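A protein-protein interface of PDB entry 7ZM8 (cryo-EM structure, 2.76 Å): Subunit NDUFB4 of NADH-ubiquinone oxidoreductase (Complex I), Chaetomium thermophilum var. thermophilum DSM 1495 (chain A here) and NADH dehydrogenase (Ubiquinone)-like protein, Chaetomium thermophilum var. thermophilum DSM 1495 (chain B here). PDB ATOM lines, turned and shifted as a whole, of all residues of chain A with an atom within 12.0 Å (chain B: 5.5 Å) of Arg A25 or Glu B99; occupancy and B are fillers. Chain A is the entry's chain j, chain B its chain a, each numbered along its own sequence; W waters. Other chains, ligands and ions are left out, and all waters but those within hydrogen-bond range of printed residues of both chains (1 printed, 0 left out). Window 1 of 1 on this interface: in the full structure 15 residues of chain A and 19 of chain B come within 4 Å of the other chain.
CG2 of Val B97 touches O of Ala A14 (3.8 Å).
Val B97 touches Leu A15 (CG1 to CD2, 3.8 Å).
Leu A18 touches Tyr B67 (CD1 to OH, 3.8 Å).
Met A21 touches Asn B64.
Met A21 touches Tyr B67 (CG to CD1, 3.7 Å).
Met B63 touches Arg A25 (O to CZ, 3.97 Å).
Phe A29 touches Met B63 (CD1 to CE, 3.3 Å).
Met B63 touches Arg A30 (CE to N, 3.2 Å).
Thr A32 touches Met B63.
Met B63 touches Thr A35.
Arg A25 touches four residues of chain B.
Of chain A, only Leu A18, Met A21 and Arg A25 come within 4 Å of Glu B99.
Asn B64 touches three residues of chain A.
Of chain A, only Leu A18 and Met A21 come within 4 Å of Tyr B67.
His B98 touches none of the printed residues of chain A.
No residue of chain A comes within 4 Å of Asp B100.
Of the printed residues of chain B, Met A21 touches Asn B64, Tyr B67 and Glu B99.
Of the printed residues of chain B, Thr A32 touches Met B63 (3.996 Å).
Of the printed residues of chain B, Tyr A28 touches Met B63 (3.9 Å) and Asn B64 (3.9 Å).
Of the printed residues of chain A, Met B63 touches Arg A25 (3.97 Å), Tyr A28 (3.9 Å), Phe A29 (3.3 Å), Arg A30 (3.2 Å), Thr A32 (3.996 Å) and Thr A35 (3.8 Å).
Printed residues of chain B within 4 Å of Leu A18: Tyr B67 (3.8 Å), Val B97 (3.7 Å) and Glu B99 (3.9 Å).
Trp A31 touches none of the printed residues of chain B.
The nearest printed residue of chain B that does not touch Arg A25 is Tyr B67 (7.1 Å).
The nearest printed residue of chain B that does not touch Thr A32 is Asp B62 (8.7 Å).
N of Tyr B67 lies within hydrogen-bond range of OD1 of Asn B64 (3.4 Å).
The side-chain amide nitrogen (ND2) of Asn B64 is in hydrogen-bond range of the side-chain carboxylate (OE1) of Glu B99 (3.4 Å).
The backbone carbonyl oxygen (O) of Val B97 is in hydrogen-bond range of the side-chain hydroxyl (OH) of Tyr B67.
N of Glu B99 is in hydrogen-bond range of OD1 of Asn B69 (3.1 Å).
The backbone carbonyl oxygen (O) of Arg A30 is in hydrogen-bond range of the side-chain hydroxyl (OG1) of Thr A35 (3.1 Å).
The backbone NH of Thr A35 sits at hydrogen-bond distance from the side-chain hydroxyl of Thr A32, 2.9 Å away.
Along chain A the printed residues that touch a printed residue of chain B span positions 14 to 35.
Of the 12 printed residues of chain B, 6 touch a printed residue of chain A.
Printed residues of chain B that touch a printed residue of chain A: Asp B62, Met B63, Asn B64, Tyr B67, Val B97 and Glu B99.
Hydrophobic or aromatic side chains of chain B that line the printed part of chain A: Met B63, Tyr B67 and Val B97.
Along chain B the printed residues that touch a printed residue of chain A span positions 62 to 99.
Among the printed residues, 18 pairs touch across the chains.
Water W1 lies within hydrogen-bond range of O of Asn B64 and O of Met A21.
The guanidinium group (NH1) of Arg A25 sits at hydrogen-bond distance from the backbone carbonyl oxygen (O) of Asp B62, at 3.4 Å.
The side-chain carboxylate (OE1) of Glu B99 is in salt-bridge range of the guanidinium group (NH2) of Arg A25, 3.4 Å away.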
ATOM      1  N   ALA A  14      -2.618  -6.345  25.038  1.00  0.00           N
ATOM      2  CA  ALA A  14      -2.391  -7.526  24.216  1.00  0.00           C
ATOM      3  C   ALA A  14      -3.668  -7.981  23.528  1.00  0.00           C
ATOM      4  O   ALA A  14      -3.641  -8.381  22.361  1.00  0.00           O
ATOM      5  CB  ALA A  14      -1.816  -8.650  25.074  1.00  0.00           C
ATOM      6  N   LEU A  15      -4.793  -7.952  24.240  1.00  0.00           N
ATOM      7  CA  LEU A  15      -6.057  -8.344  23.630  1.00  0.00           C
ATOM      8  C   LEU A  15      -6.585  -7.268  22.694  1.00  0.00           C
ATOM      9  O   LEU A  15      -7.273  -7.583  21.719  1.00  0.00           O
ATOM     10  CB  LEU A  15      -7.081  -8.661  24.714  1.00  0.00           C
ATOM     11  CG  LEU A  15      -6.644  -9.699  25.741  1.00  0.00           C
ATOM     12  CD1 LEU A  15      -7.626  -9.739  26.887  1.00  0.00           C
ATOM     13  CD2 LEU A  15      -6.533 -11.058  25.094  1.00  0.00           C
ATOM     14  N   VAL A  16      -6.290  -5.999  22.978  1.00  0.00           N
ATOM     15  CA  VAL A  16      -6.724  -4.922  22.094  1.00  0.00           C
ATOM     16  C   VAL A  16      -6.013  -5.010  20.751  1.00  0.00           C
ATOM     17  O   VAL A  16      -6.633  -4.847  19.694  1.00  0.00           O
ATOM     18  CB  VAL A  16      -6.506  -3.558  22.773  1.00  0.00           C
ATOM     19  CG1 VAL A  16      -6.518  -2.442  21.757  1.00  0.00           C
ATOM     20  CG2 VAL A  16      -7.577  -3.320  23.815  1.00  0.00           C
ATOM     21  N   ARG A  17      -4.707  -5.273  20.763  1.00  0.00           N
ATOM     22  CA  ARG A  17      -3.984  -5.398  19.505  1.00  0.00           C
ATOM     23  C   ARG A  17      -4.342  -6.687  18.777  1.00  0.00           C
ATOM     24  O   ARG A  17      -4.254  -6.741  17.547  1.00  0.00           O
ATOM     25  CB  ARG A  17      -2.478  -5.309  19.749  1.00  0.00           C
ATOM     26  CG  ARG A  17      -1.880  -6.464  20.503  1.00  0.00           C
ATOM     27  CD  ARG A  17      -0.375  -6.475  20.368  1.00  0.00           C
ATOM     28  NE  ARG A  17       0.282  -6.979  21.570  1.00  0.00           N
ATOM     29  CZ  ARG A  17       0.694  -6.214  22.575  1.00  0.00           C
ATOM     30  NH1 ARG A  17       1.280  -6.763  23.629  1.00  0.00           N
ATOM     31  NH2 ARG A  17       0.518  -4.901  22.529  1.00  0.00           N
ATOM     32  N   LEU A  18      -4.745  -7.728  19.510  1.00  0.00           N
ATOM     33  CA  LEU A  18      -5.241  -8.941  18.872  1.00  0.00           C
ATOM     34  C   LEU A  18      -6.563  -8.695  18.160  1.00  0.00           C
ATOM     35  O   LEU A  18      -6.756  -9.142  17.026  1.00  0.00           O
ATOM     36  CB  LEU A  18      -5.403 -10.052  19.905  1.00  0.00           C
ATOM     37  CG  LEU A  18      -6.074 -11.329  19.400  1.00  0.00           C
ATOM     38  CD1 LEU A  18      -5.239 -12.003  18.342  1.00  0.00           C
ATOM     39  CD2 LEU A  18      -6.369 -12.271  20.540  1.00  0.00           C
ATOM     40  N   GLY A  19      -7.492  -8.006  18.817  1.00  0.00           N
ATOM     41  CA  GLY A  19      -8.746  -7.675  18.168  1.00  0.00           C
ATOM     42  C   GLY A  19      -8.559  -6.749  16.988  1.00  0.00           C
ATOM     43  O   GLY A  19      -9.295  -6.833  16.004  1.00  0.00           O
ATOM     44  N   SER A  20      -7.583  -5.846  17.075  1.00  0.00           N
ATOM     45  CA  SER A  20      -7.220  -5.036  15.921  1.00  0.00           C
ATOM     46  C   SER A  20      -6.655  -5.900  14.803  1.00  0.00           C
ATOM     47  O   SER A  20      -6.935  -5.659  13.625  1.00  0.00           O
ATOM     48  CB  SER A  20      -6.217  -3.963  16.335  1.00  0.00           C
ATOM     49  OG  SER A  20      -6.800  -3.062  17.255  1.00  0.00           O
ATOM     50  N   MET A  21      -5.852  -6.905  15.153  1.00  0.00           N
ATOM     51  CA  MET A  21      -5.286  -7.786  14.139  1.00  0.00           C
ATOM     52  C   MET A  21      -6.379  -8.533  13.393  1.00  0.00           C
ATOM     53  O   MET A  21      -6.325  -8.664  12.165  1.00  0.00           O
ATOM     54  CB  MET A  21      -4.307  -8.764  14.788  1.00  0.00           C
ATOM     55  CG  MET A  21      -3.495  -9.605  13.811  1.00  0.00           C
ATOM     56  SD  MET A  21      -4.334 -11.095  13.229  1.00  0.00           S
ATOM     57  CE  MET A  21      -4.261 -12.117  14.690  1.00  0.00           C
ATOM     58  N   ILE A  22      -7.360  -9.061  14.109  1.00  0.00           N
ATOM     59  CA  ILE A  22      -8.431  -9.864  13.456  1.00  0.00           C
ATOM     60  C   ILE A  22      -9.191  -8.952  12.481  1.00  0.00           C
ATOM     61  O   ILE A  22      -9.450  -9.387  11.351  1.00  0.00           O
ATOM     62  CB  ILE A  22      -9.296 -10.523  14.546  1.00  0.00           C
ATOM     63  CG1 ILE A  22      -8.515 -11.636  15.245  1.00  0.00           C
ATOM     64  CG2 ILE A  22     -10.606 -11.034  13.978  1.00  0.00           C
ATOM     65  CD1 ILE A  22      -9.197 -12.214  16.459  1.00  0.00           C
ATOM     66  N   SER A  23      -9.459  -7.709  12.870  1.00  0.00           N
ATOM     67  CA  SER A  23     -10.219  -6.741  12.037  1.00  0.00           C
ATOM     68  C   SER A  23      -9.505  -6.348  10.743  1.00  0.00           C
ATOM     69  O   SER A  23     -10.204  -6.199   9.732  1.00  0.00           O
ATOM     70  CB  SER A  23     -10.555  -5.519  12.833  1.00  0.00           C
ATOM     71  OG  SER A  23     -11.384  -5.856  13.934  1.00  0.00           O
ATOM     72  N   ASN A  24      -8.191  -6.187  10.744  1.00  0.00           N
ATOM     73  CA  ASN A  24      -7.503  -5.682   9.534  1.00  0.00           C
ATOM     74  C   ASN A  24      -6.875  -6.833   8.758  1.00  0.00           C
ATOM     75  O   ASN A  24      -6.347  -6.570   7.689  1.00  0.00           O
ATOM     76  CB  ASN A  24      -6.470  -4.639   9.948  1.00  0.00           C
ATOM     77  CG  ASN A  24      -7.094  -3.398  10.543  1.00  0.00           C
ATOM     78  OD1 ASN A  24      -7.714  -2.613   9.833  1.00  0.00           O
ATOM     79  ND2 ASN A  24      -6.924  -3.204  11.839  1.00  0.00           N
ATOM     80  N   ARG A  25      -6.994  -8.071   9.230  1.00  0.00           N
ATOM     81  CA  ARG A  25      -6.335  -9.279   8.647  1.00  0.00           C
ATOM     82  C   ARG A  25      -6.478  -9.423   7.126  1.00  0.00           C
ATOM     83  O   ARG A  25      -5.512  -9.881   6.508  1.00  0.00           O
ATOM     84  CB  ARG A  25      -6.874 -10.504   9.393  1.00  0.00           C
ATOM     85  CG  ARG A  25      -6.169 -11.806   9.056  1.00  0.00           C
ATOM     86  CD  ARG A  25      -6.869 -13.033   9.600  1.00  0.00           C
ATOM     87  NE  ARG A  25      -6.223 -14.201   9.029  1.00  0.00           N
ATOM     88  CZ  ARG A  25      -5.234 -14.873   9.598  1.00  0.00           C
ATOM     89  NH1 ARG A  25      -4.710 -15.916   8.982  1.00  0.00           N
ATOM     90  NH2 ARG A  25      -4.789 -14.520  10.789  1.00  0.00           N
ATOM     91  N   TYR A  26      -7.629  -9.084   6.558  1.00  0.00           N
ATOM     92  CA  TYR A  26      -7.892  -9.277   5.108  1.00  0.00           C
ATOM     93  C   TYR A  26      -6.880  -8.486   4.274  1.00  0.00           C
ATOM     94  O   TYR A  26      -6.508  -8.934   3.193  1.00  0.00           O
ATOM     95  CB  TYR A  26      -9.341  -8.876   4.794  1.00  0.00           C
ATOM     96  CG  TYR A  26      -9.625  -7.401   4.906  1.00  0.00           C
ATOM     97  CD1 TYR A  26      -9.833  -6.806   6.138  1.00  0.00           C
ATOM     98  CD2 TYR A  26      -9.666  -6.593   3.782  1.00  0.00           C
ATOM     99  CE1 TYR A  26     -10.077  -5.450   6.254  1.00  0.00           C
ATOM    100  CE2 TYR A  26      -9.909  -5.235   3.880  1.00  0.00           C
ATOM    101  CZ  TYR A  26     -10.112  -4.660   5.121  1.00  0.00           C
ATOM    102  OH  TYR A  26     -10.354  -3.323   5.230  1.00  0.00           O
ATOM    103  N   LYS A  27      -6.493  -7.316   4.743  1.00  0.00           N
ATOM    104  CA  LYS A  27      -5.516  -6.475   4.034  1.00  0.00           C
ATOM    105  C   LYS A  27      -4.224  -7.262   3.803  1.00  0.00           C
ATOM    106  O   LYS A  27      -3.388  -6.767   3.032  1.00  0.00           O
ATOM    107  CB  LYS A  27      -5.276  -5.230   4.882  1.00  0.00           C
ATOM    108  CG  LYS A  27      -6.398  -4.207   4.893  1.00  0.00           C
ATOM    109  CD  LYS A  27      -6.333  -3.293   6.089  1.00  0.00           C
ATOM    110  CE  LYS A  27      -4.919  -2.899   6.451  1.00  0.00           C
ATOM    111  NZ  LYS A  27      -4.885  -2.018   7.642  1.00  0.00           N
ATOM    112  N   TYR A  28      -4.066  -8.450   4.410  1.00  0.00           N
ATOM    113  CA  TYR A  28      -2.798  -9.124   4.174  1.00  0.00           C
ATOM    114  C   TYR A  28      -2.953 -10.508   3.562  1.00  0.00           C
ATOM    115  O   TYR A  28      -1.976 -11.258   3.512  1.00  0.00           O
ATOM    116  CB  TYR A  28      -1.985  -9.217   5.465  1.00  0.00           C
ATOM    117  CG  TYR A  28      -1.879  -7.920   6.226  1.00  0.00           C
ATOM    118  CD1 TYR A  28      -2.928  -7.451   7.000  1.00  0.00           C
ATOM    119  CD2 TYR A  28      -0.745  -7.133   6.121  1.00  0.00           C
ATOM    120  CE1 TYR A  28      -2.833  -6.268   7.677  1.00  0.00           C
ATOM    121  CE2 TYR A  28      -0.645  -5.947   6.791  1.00  0.00           C
ATOM    122  CZ  TYR A  28      -1.689  -5.518   7.566  1.00  0.00           C
ATOM    123  OH  TYR A  28      -1.584  -4.324   8.238  1.00  0.00           O
ATOM    124  N   PHE A  29      -4.134 -10.863   3.077  1.00  0.00           N
ATOM    125  CA  PHE A  29      -4.302 -12.149   2.417  1.00  0.00           C
ATOM    126  C   PHE A  29      -3.601 -12.147   1.065  1.00  0.00           C
ATOM    127  O   PHE A  29      -3.729 -11.206   0.279  1.00  0.00           O
ATOM    128  CB  PHE A  29      -5.787 -12.472   2.245  1.00  0.00           C
ATOM    129  CG  PHE A  29      -6.050 -13.757   1.509  1.00  0.00           C
ATOM    130  CD1 PHE A  29      -6.099 -14.959   2.179  1.00  0.00           C
ATOM    131  CD2 PHE A  29      -6.257 -13.756   0.147  1.00  0.00           C
ATOM    132  CE1 PHE A  29      -6.334 -16.125   1.514  1.00  0.00           C
ATOM    133  CE2 PHE A  29      -6.488 -14.923  -0.527  1.00  0.00           C
ATOM    134  CZ  PHE A  29      -6.532 -16.111   0.159  1.00  0.00           C
ATOM    135  N   ARG A  30      -2.867 -13.220   0.790  1.00  0.00           N
ATOM    136  CA  ARG A  30      -2.172 -13.387  -0.471  1.00  0.00           C
ATOM    137  C   ARG A  30      -2.683 -14.643  -1.157  1.00  0.00           C
ATOM    138  O   ARG A  30      -3.287 -15.514  -0.530  1.00  0.00           O
ATOM    139  CB  ARG A  30      -0.664 -13.530  -0.283  1.00  0.00           C
ATOM    140  CG  ARG A  30       0.074 -12.323   0.210  1.00  0.00           C
ATOM    141  CD  ARG A  30       1.551 -12.622   0.118  1.00  0.00           C
ATOM    142  NE  ARG A  30       1.918 -13.733   0.989  1.00  0.00           N
ATOM    143  CZ  ARG A  30       2.263 -13.616   2.261  1.00  0.00           C
ATOM    144  NH1 ARG A  30       2.292 -12.426   2.834  1.00  0.00           N
ATOM    145  NH2 ARG A  30       2.569 -14.694   2.961  1.00  0.00           N
ATOM    146  N   TRP A  31      -2.353 -14.771  -2.440  1.00  0.00           N
ATOM    147  CA  TRP A  31      -2.694 -16.007  -3.184  1.00  0.00           C
ATOM    148  C   TRP A  31      -1.447 -16.875  -3.191  1.00  0.00           C
ATOM    149  O   TRP A  31      -0.495 -16.521  -3.897  1.00  0.00           O
ATOM    150  CB  TRP A  31      -3.132 -15.721  -4.623  1.00  0.00           C
ATOM    151  CG  TRP A  31      -4.541 -15.254  -4.799  1.00  0.00           C
ATOM    152  CD1 TRP A  31      -4.949 -14.057  -5.308  1.00  0.00           C
ATOM    153  CD2 TRP A  31      -5.736 -15.990  -4.496  1.00  0.00           C
ATOM    154  NE1 TRP A  31      -6.314 -13.991  -5.329  1.00  0.00           N
ATOM    155  CE2 TRP A  31      -6.826 -15.160  -4.834  1.00  0.00           C
ATOM    156  CE3 TRP A  31      -5.992 -17.257  -3.963  1.00  0.00           C
ATOM    157  CZ2 TRP A  31      -8.148 -15.562  -4.658  1.00  0.00           C
ATOM    158  CZ3 TRP A  31      -7.298 -17.655  -3.791  1.00  0.00           C
ATOM    159  CH2 TRP A  31      -8.358 -16.818  -4.138  1.00  0.00           C
ATOM    160  N   THR A  32      -1.439 -17.938  -2.404  1.00  0.00           N
ATOM    161  CA  THR A  32      -0.355 -18.895  -2.335  1.00  0.00           C
ATOM    162  C   THR A  32      -0.833 -20.214  -2.919  1.00  0.00           C
ATOM    163  O   THR A  32      -1.977 -20.343  -3.357  1.00  0.00           O
ATOM    164  CB  THR A  32       0.137 -19.079  -0.895  1.00  0.00           C
ATOM    165  OG1 THR A  32      -0.817 -19.842  -0.152  1.00  0.00           O
ATOM    166  CG2 THR A  32       0.331 -17.739  -0.220  1.00  0.00           C
ATOM    167  N   ARG A  34      -1.118 -22.675  -0.986  1.00  0.00           N
ATOM    168  CA  ARG A  34      -1.913 -23.210   0.109  1.00  0.00           C
ATOM    169  C   ARG A  34      -3.290 -22.561   0.167  1.00  0.00           C
ATOM    170  O   ARG A  34      -4.303 -23.254   0.293  1.00  0.00           O
ATOM    171  CB  ARG A  34      -1.169 -23.015   1.432  1.00  0.00           C
ATOM    172  CG  ARG A  34      -1.723 -23.823   2.588  1.00  0.00           C
ATOM    173  CD  ARG A  34      -1.281 -23.240   3.918  1.00  0.00           C
ATOM    174  NE  ARG A  34      -2.192 -23.585   5.004  1.00  0.00           N
ATOM    175  CZ  ARG A  34      -3.134 -22.774   5.475  1.00  0.00           C
ATOM    176  NH1 ARG A  34      -3.293 -21.565   4.953  1.00  0.00           N
ATOM    177  NH2 ARG A  34      -3.917 -23.174   6.468  1.00  0.00           N
ATOM    178  N   THR A  35      -3.345 -21.230   0.084  1.00  0.00           N
ATOM    179  CA  THR A  35      -4.624 -20.541   0.209  1.00  0.00           C
ATOM    180  C   THR A  35      -5.533 -20.862  -0.968  1.00  0.00           C
ATOM    181  O   THR A  35      -6.756 -20.929  -0.817  1.00  0.00           O
ATOM    182  CB  THR A  35      -4.407 -19.034   0.326  1.00  0.00           C
ATOM    183  OG1 THR A  35      -3.827 -18.538  -0.882  1.00  0.00           O
ATOM    184  CG2 THR A  35      -3.491 -18.720   1.477  1.00  0.00           C
ATOM    185  N   VAL A  38      -7.000 -24.481  -0.234  1.00  0.00           N
ATOM    186  CA  VAL A  38      -8.110 -24.444   0.712  1.00  0.00           C
ATOM    187  C   VAL A  38      -9.319 -23.749   0.093  1.00  0.00           C
ATOM    188  O   VAL A  38     -10.462 -24.180   0.275  1.00  0.00           O
ATOM    189  CB  VAL A  38      -7.667 -23.772   2.024  1.00  0.00           C
ATOM    190  CG1 VAL A  38      -8.852 -23.454   2.900  1.00  0.00           C
ATOM    191  CG2 VAL A  38      -6.704 -24.662   2.773  1.00  0.00           C
ATOM    192  N   SER A  39      -9.089 -22.669  -0.651  1.00  0.00           N
ATOM    193  CA  SER A  39     -10.201 -21.938  -1.245  1.00  0.00           C
ATOM    194  C   SER A  39     -10.909 -22.768  -2.304  1.00  0.00           C
ATOM    195  O   SER A  39     -12.143 -22.773  -2.373  1.00  0.00           O
ATOM    196  CB  SER A  39      -9.701 -20.626  -1.839  1.00  0.00           C
ATOM    197  OG  SER A  39      -8.851 -19.969  -0.921  1.00  0.00           O
ATOM    198  N   ASP B  62       2.199 -15.782   8.360  1.00  0.00           N
ATOM    199  CA  ASP B  62       0.860 -16.118   8.816  1.00  0.00           C
ATOM    200  C   ASP B  62      -0.220 -15.340   8.081  1.00  0.00           C
ATOM    201  O   ASP B  62      -1.405 -15.597   8.314  1.00  0.00           O
ATOM    202  CB  ASP B  62       0.745 -15.871  10.319  1.00  0.00           C
ATOM    203  CG  ASP B  62       1.570 -16.845  11.130  1.00  0.00           C
ATOM    204  OD1 ASP B  62       1.770 -17.984  10.661  1.00  0.00           O
ATOM    205  OD2 ASP B  62       2.024 -16.475  12.234  1.00  0.00           O
ATOM    206  N   MET B  63       0.163 -14.408   7.209  1.00  0.00           N
ATOM    207  CA  MET B  63      -0.784 -13.700   6.355  1.00  0.00           C
ATOM    208  C   MET B  63      -1.819 -12.961   7.200  1.00  0.00           C
ATOM    209  O   MET B  63      -3.019 -12.965   6.915  1.00  0.00           O
ATOM    210  CB  MET B  63      -1.429 -14.680   5.375  1.00  0.00           C
ATOM    211  CG  MET B  63      -0.556 -14.954   4.166  1.00  0.00           C
ATOM    212  SD  MET B  63      -1.362 -15.972   2.939  1.00  0.00           S
ATOM    213  CE  MET B  63      -3.005 -15.359   3.132  1.00  0.00           C
ATOM    214  N   ASN B  64      -1.325 -12.322   8.261  1.00  0.00           N
ATOM    215  CA  ASN B  64      -2.159 -11.641   9.237  1.00  0.00           C
ATOM    216  C   ASN B  64      -1.715 -10.213   9.518  1.00  0.00           C
ATOM    217  O   ASN B  64      -2.417  -9.497  10.238  1.00  0.00           O
ATOM    218  CB  ASN B  64      -2.183 -12.426  10.555  1.00  0.00           C
ATOM    219  CG  ASN B  64      -0.802 -12.618  11.143  1.00  0.00           C
ATOM    220  OD1 ASN B  64       0.190 -12.139  10.604  1.00  0.00           O
ATOM    221  ND2 ASN B  64      -0.732 -13.335  12.251  1.00  0.00           N
ATOM    222  N   TYR B  67       1.811 -10.011  12.631  1.00  0.00           N
ATOM    223  CA  TYR B  67       1.559 -10.256  14.042  1.00  0.00           C
ATOM    224  C   TYR B  67       2.482 -11.342  14.569  1.00  0.00           C
ATOM    225  O   TYR B  67       2.499 -12.460  14.051  1.00  0.00           O
ATOM    226  CB  TYR B  67       0.094 -10.655  14.223  1.00  0.00           C
ATOM    227  CG  TYR B  67      -0.353 -10.902  15.642  1.00  0.00           C
ATOM    228  CD1 TYR B  67      -0.829  -9.866  16.429  1.00  0.00           C
ATOM    229  CD2 TYR B  67      -0.326 -12.174  16.185  1.00  0.00           C
ATOM    230  CE1 TYR B  67      -1.251 -10.090  17.722  1.00  0.00           C
ATOM    231  CE2 TYR B  67      -0.746 -12.408  17.468  1.00  0.00           C
ATOM    232  CZ  TYR B  67      -1.208 -11.364  18.236  1.00  0.00           C
ATOM    233  OH  TYR B  67      -1.626 -11.599  19.523  1.00  0.00           O
ATOM    234  N   ASN B  69       3.573 -14.178  17.055  1.00  0.00           N
ATOM    235  CA  ASN B  69       2.668 -15.159  17.629  1.00  0.00           C
ATOM    236  C   ASN B  69       3.393 -15.998  18.672  1.00  0.00           C
ATOM    237  O   ASN B  69       4.455 -16.566  18.371  1.00  0.00           O
ATOM    238  CB  ASN B  69       2.108 -16.049  16.521  1.00  0.00           C
ATOM    239  CG  ASN B  69       0.673 -16.420  16.750  1.00  0.00           C
ATOM    240  OD1 ASN B  69       0.082 -16.055  17.759  1.00  0.00           O
ATOM    241  ND2 ASN B  69       0.090 -17.130  15.799  1.00  0.00           N
ATOM    242  N   PRO B  70       2.879 -16.102  19.891  1.00  0.00           N
ATOM    243  CA  PRO B  70       3.468 -17.011  20.871  1.00  0.00           C
ATOM    244  C   PRO B  70       3.281 -18.456  20.444  1.00  0.00           C
ATOM    245  O   PRO B  70       2.562 -18.736  19.476  1.00  0.00           O
ATOM    246  CB  PRO B  70       2.678 -16.703  22.152  1.00  0.00           C
ATOM    247  CG  PRO B  70       2.149 -15.341  21.948  1.00  0.00           C
ATOM    248  CD  PRO B  70       1.839 -15.255  20.492  1.00  0.00           C
ATOM    249  N   VAL B  97      -0.715 -12.976  23.465  1.00  0.00           N
ATOM    250  CA  VAL B  97      -1.718 -14.002  23.228  1.00  0.00           C
ATOM    251  C   VAL B  97      -1.536 -14.556  21.825  1.00  0.00           C
ATOM    252  O   VAL B  97      -1.294 -13.804  20.876  1.00  0.00           O
ATOM    253  CB  VAL B  97      -3.145 -13.448  23.425  1.00  0.00           C
ATOM    254  CG1 VAL B  97      -3.404 -13.193  24.893  1.00  0.00           C
ATOM    255  CG2 VAL B  97      -3.333 -12.175  22.646  1.00  0.00           C
ATOM    256  N   HIS B  98      -1.623 -15.876  21.701  1.00  0.00           N
ATOM    257  CA  HIS B  98      -1.687 -16.490  20.385  1.00  0.00           C
ATOM    258  C   HIS B  98      -2.986 -16.087  19.699  1.00  0.00           C
ATOM    259  O   HIS B  98      -4.001 -15.826  20.346  1.00  0.00           O
ATOM    260  CB  HIS B  98      -1.589 -18.011  20.502  1.00  0.00           C
ATOM    261  CG  HIS B  98      -1.368 -18.715  19.199  1.00  0.00           C
ATOM    262  ND1 HIS B  98      -2.397 -19.044  18.345  1.00  0.00           N
ATOM    263  CD2 HIS B  98      -0.237 -19.168  18.612  1.00  0.00           C
ATOM    264  CE1 HIS B  98      -1.909 -19.655  17.281  1.00  0.00           C
ATOM    265  NE2 HIS B  98      -0.600 -19.747  17.421  1.00  0.00           N
ATOM    266  N   GLU B  99      -2.951 -16.037  18.369  1.00  0.00           N
ATOM    267  CA  GLU B  99      -4.133 -15.633  17.618  1.00  0.00           C
ATOM    268  C   GLU B  99      -5.296 -16.593  17.812  1.00  0.00           C
ATOM    269  O   GLU B  99      -6.434 -16.248  17.476  1.00  0.00           O
ATOM    270  CB  GLU B  99      -3.798 -15.522  16.136  1.00  0.00           C
ATOM    271  CG  GLU B  99      -3.432 -16.839  15.496  1.00  0.00           C
ATOM    272  CD  GLU B  99      -3.043 -16.685  14.045  1.00  0.00           C
ATOM    273  OE1 GLU B  99      -3.037 -15.539  13.548  1.00  0.00           O
ATOM    274  OE2 GLU B  99      -2.744 -17.711  13.398  1.00  0.00           O
ATOM    275  N   ASP B 100      -5.039 -17.784  18.345  1.00  0.00           N
ATOM    276  CA  ASP B 100      -6.056 -18.801  18.587  1.00  0.00           C
ATOM    277  C   ASP B 100      -6.526 -18.784  20.032  1.00  0.00           C
ATOM    278  O   ASP B 100      -6.865 -19.820  20.598  1.00  0.00           O
ATOM    279  CB  ASP B 100      -5.516 -20.175  18.214  1.00  0.00           C
ATOM    280  CG  ASP B 100      -5.642 -20.460  16.739  1.00  0.00           C
ATOM    281  OD1 ASP B 100      -5.707 -19.498  15.953  1.00  0.00           O
ATOM    282  OD2 ASP B 100      -5.673 -21.647  16.363  1.00  0.00           O
ATOM    283  N   HIS B 101      -6.450 -17.616  20.667  1.00  0.00           N
ATOM    284  CA  HIS B 101      -6.792 -17.464  22.107  1.00  0.00           C
ATOM    285  C   HIS B 101      -8.099 -18.172  22.488  1.00  0.00           C
ATOM    286  O   HIS B 101      -8.136 -18.738  23.593  1.00  0.00           O
ATOM    287  CB  HIS B 101      -6.783 -15.962  22.438  1.00  0.00           C
ATOM    288  CG  HIS B 101      -6.802 -15.614  23.888  1.00  0.00           C
ATOM    289  ND1 HIS B 101      -5.673 -15.665  24.674  1.00  0.00           N
ATOM    290  CD2 HIS B 101      -7.795 -15.171  24.685  1.00  0.00           C
ATOM    291  CE1 HIS B 101      -5.973 -15.281  25.897  1.00  0.00           C
ATOM    292  NE2 HIS B 101      -7.268 -14.977  25.929  1.00  0.00           N
ATOM    293  N   ASP B 102      -9.123 -18.144  21.626  1.00  0.00           N
ATOM    294  CA  ASP B 102     -10.419 -18.705  21.995  1.00  0.00           C
ATOM    295  C   ASP B 102     -10.288 -20.144  22.464  1.00  0.00           C
ATOM    296  O   ASP B 102     -10.773 -20.511  23.540  1.00  0.00           O
ATOM    297  CB  ASP B 102     -11.376 -18.649  20.806  1.00  0.00           C
ATOM    298  CG  ASP B 102     -11.384 -17.306  20.128  1.00  0.00           C
ATOM    299  OD1 ASP B 102     -11.545 -16.293  20.831  1.00  0.00           O
ATOM    300  OD2 ASP B 102     -11.228 -17.266  18.889  1.00  0.00           O
HETATM  301  O   HOH W   1      -3.925  -7.462  11.085  1.00  0.00           O
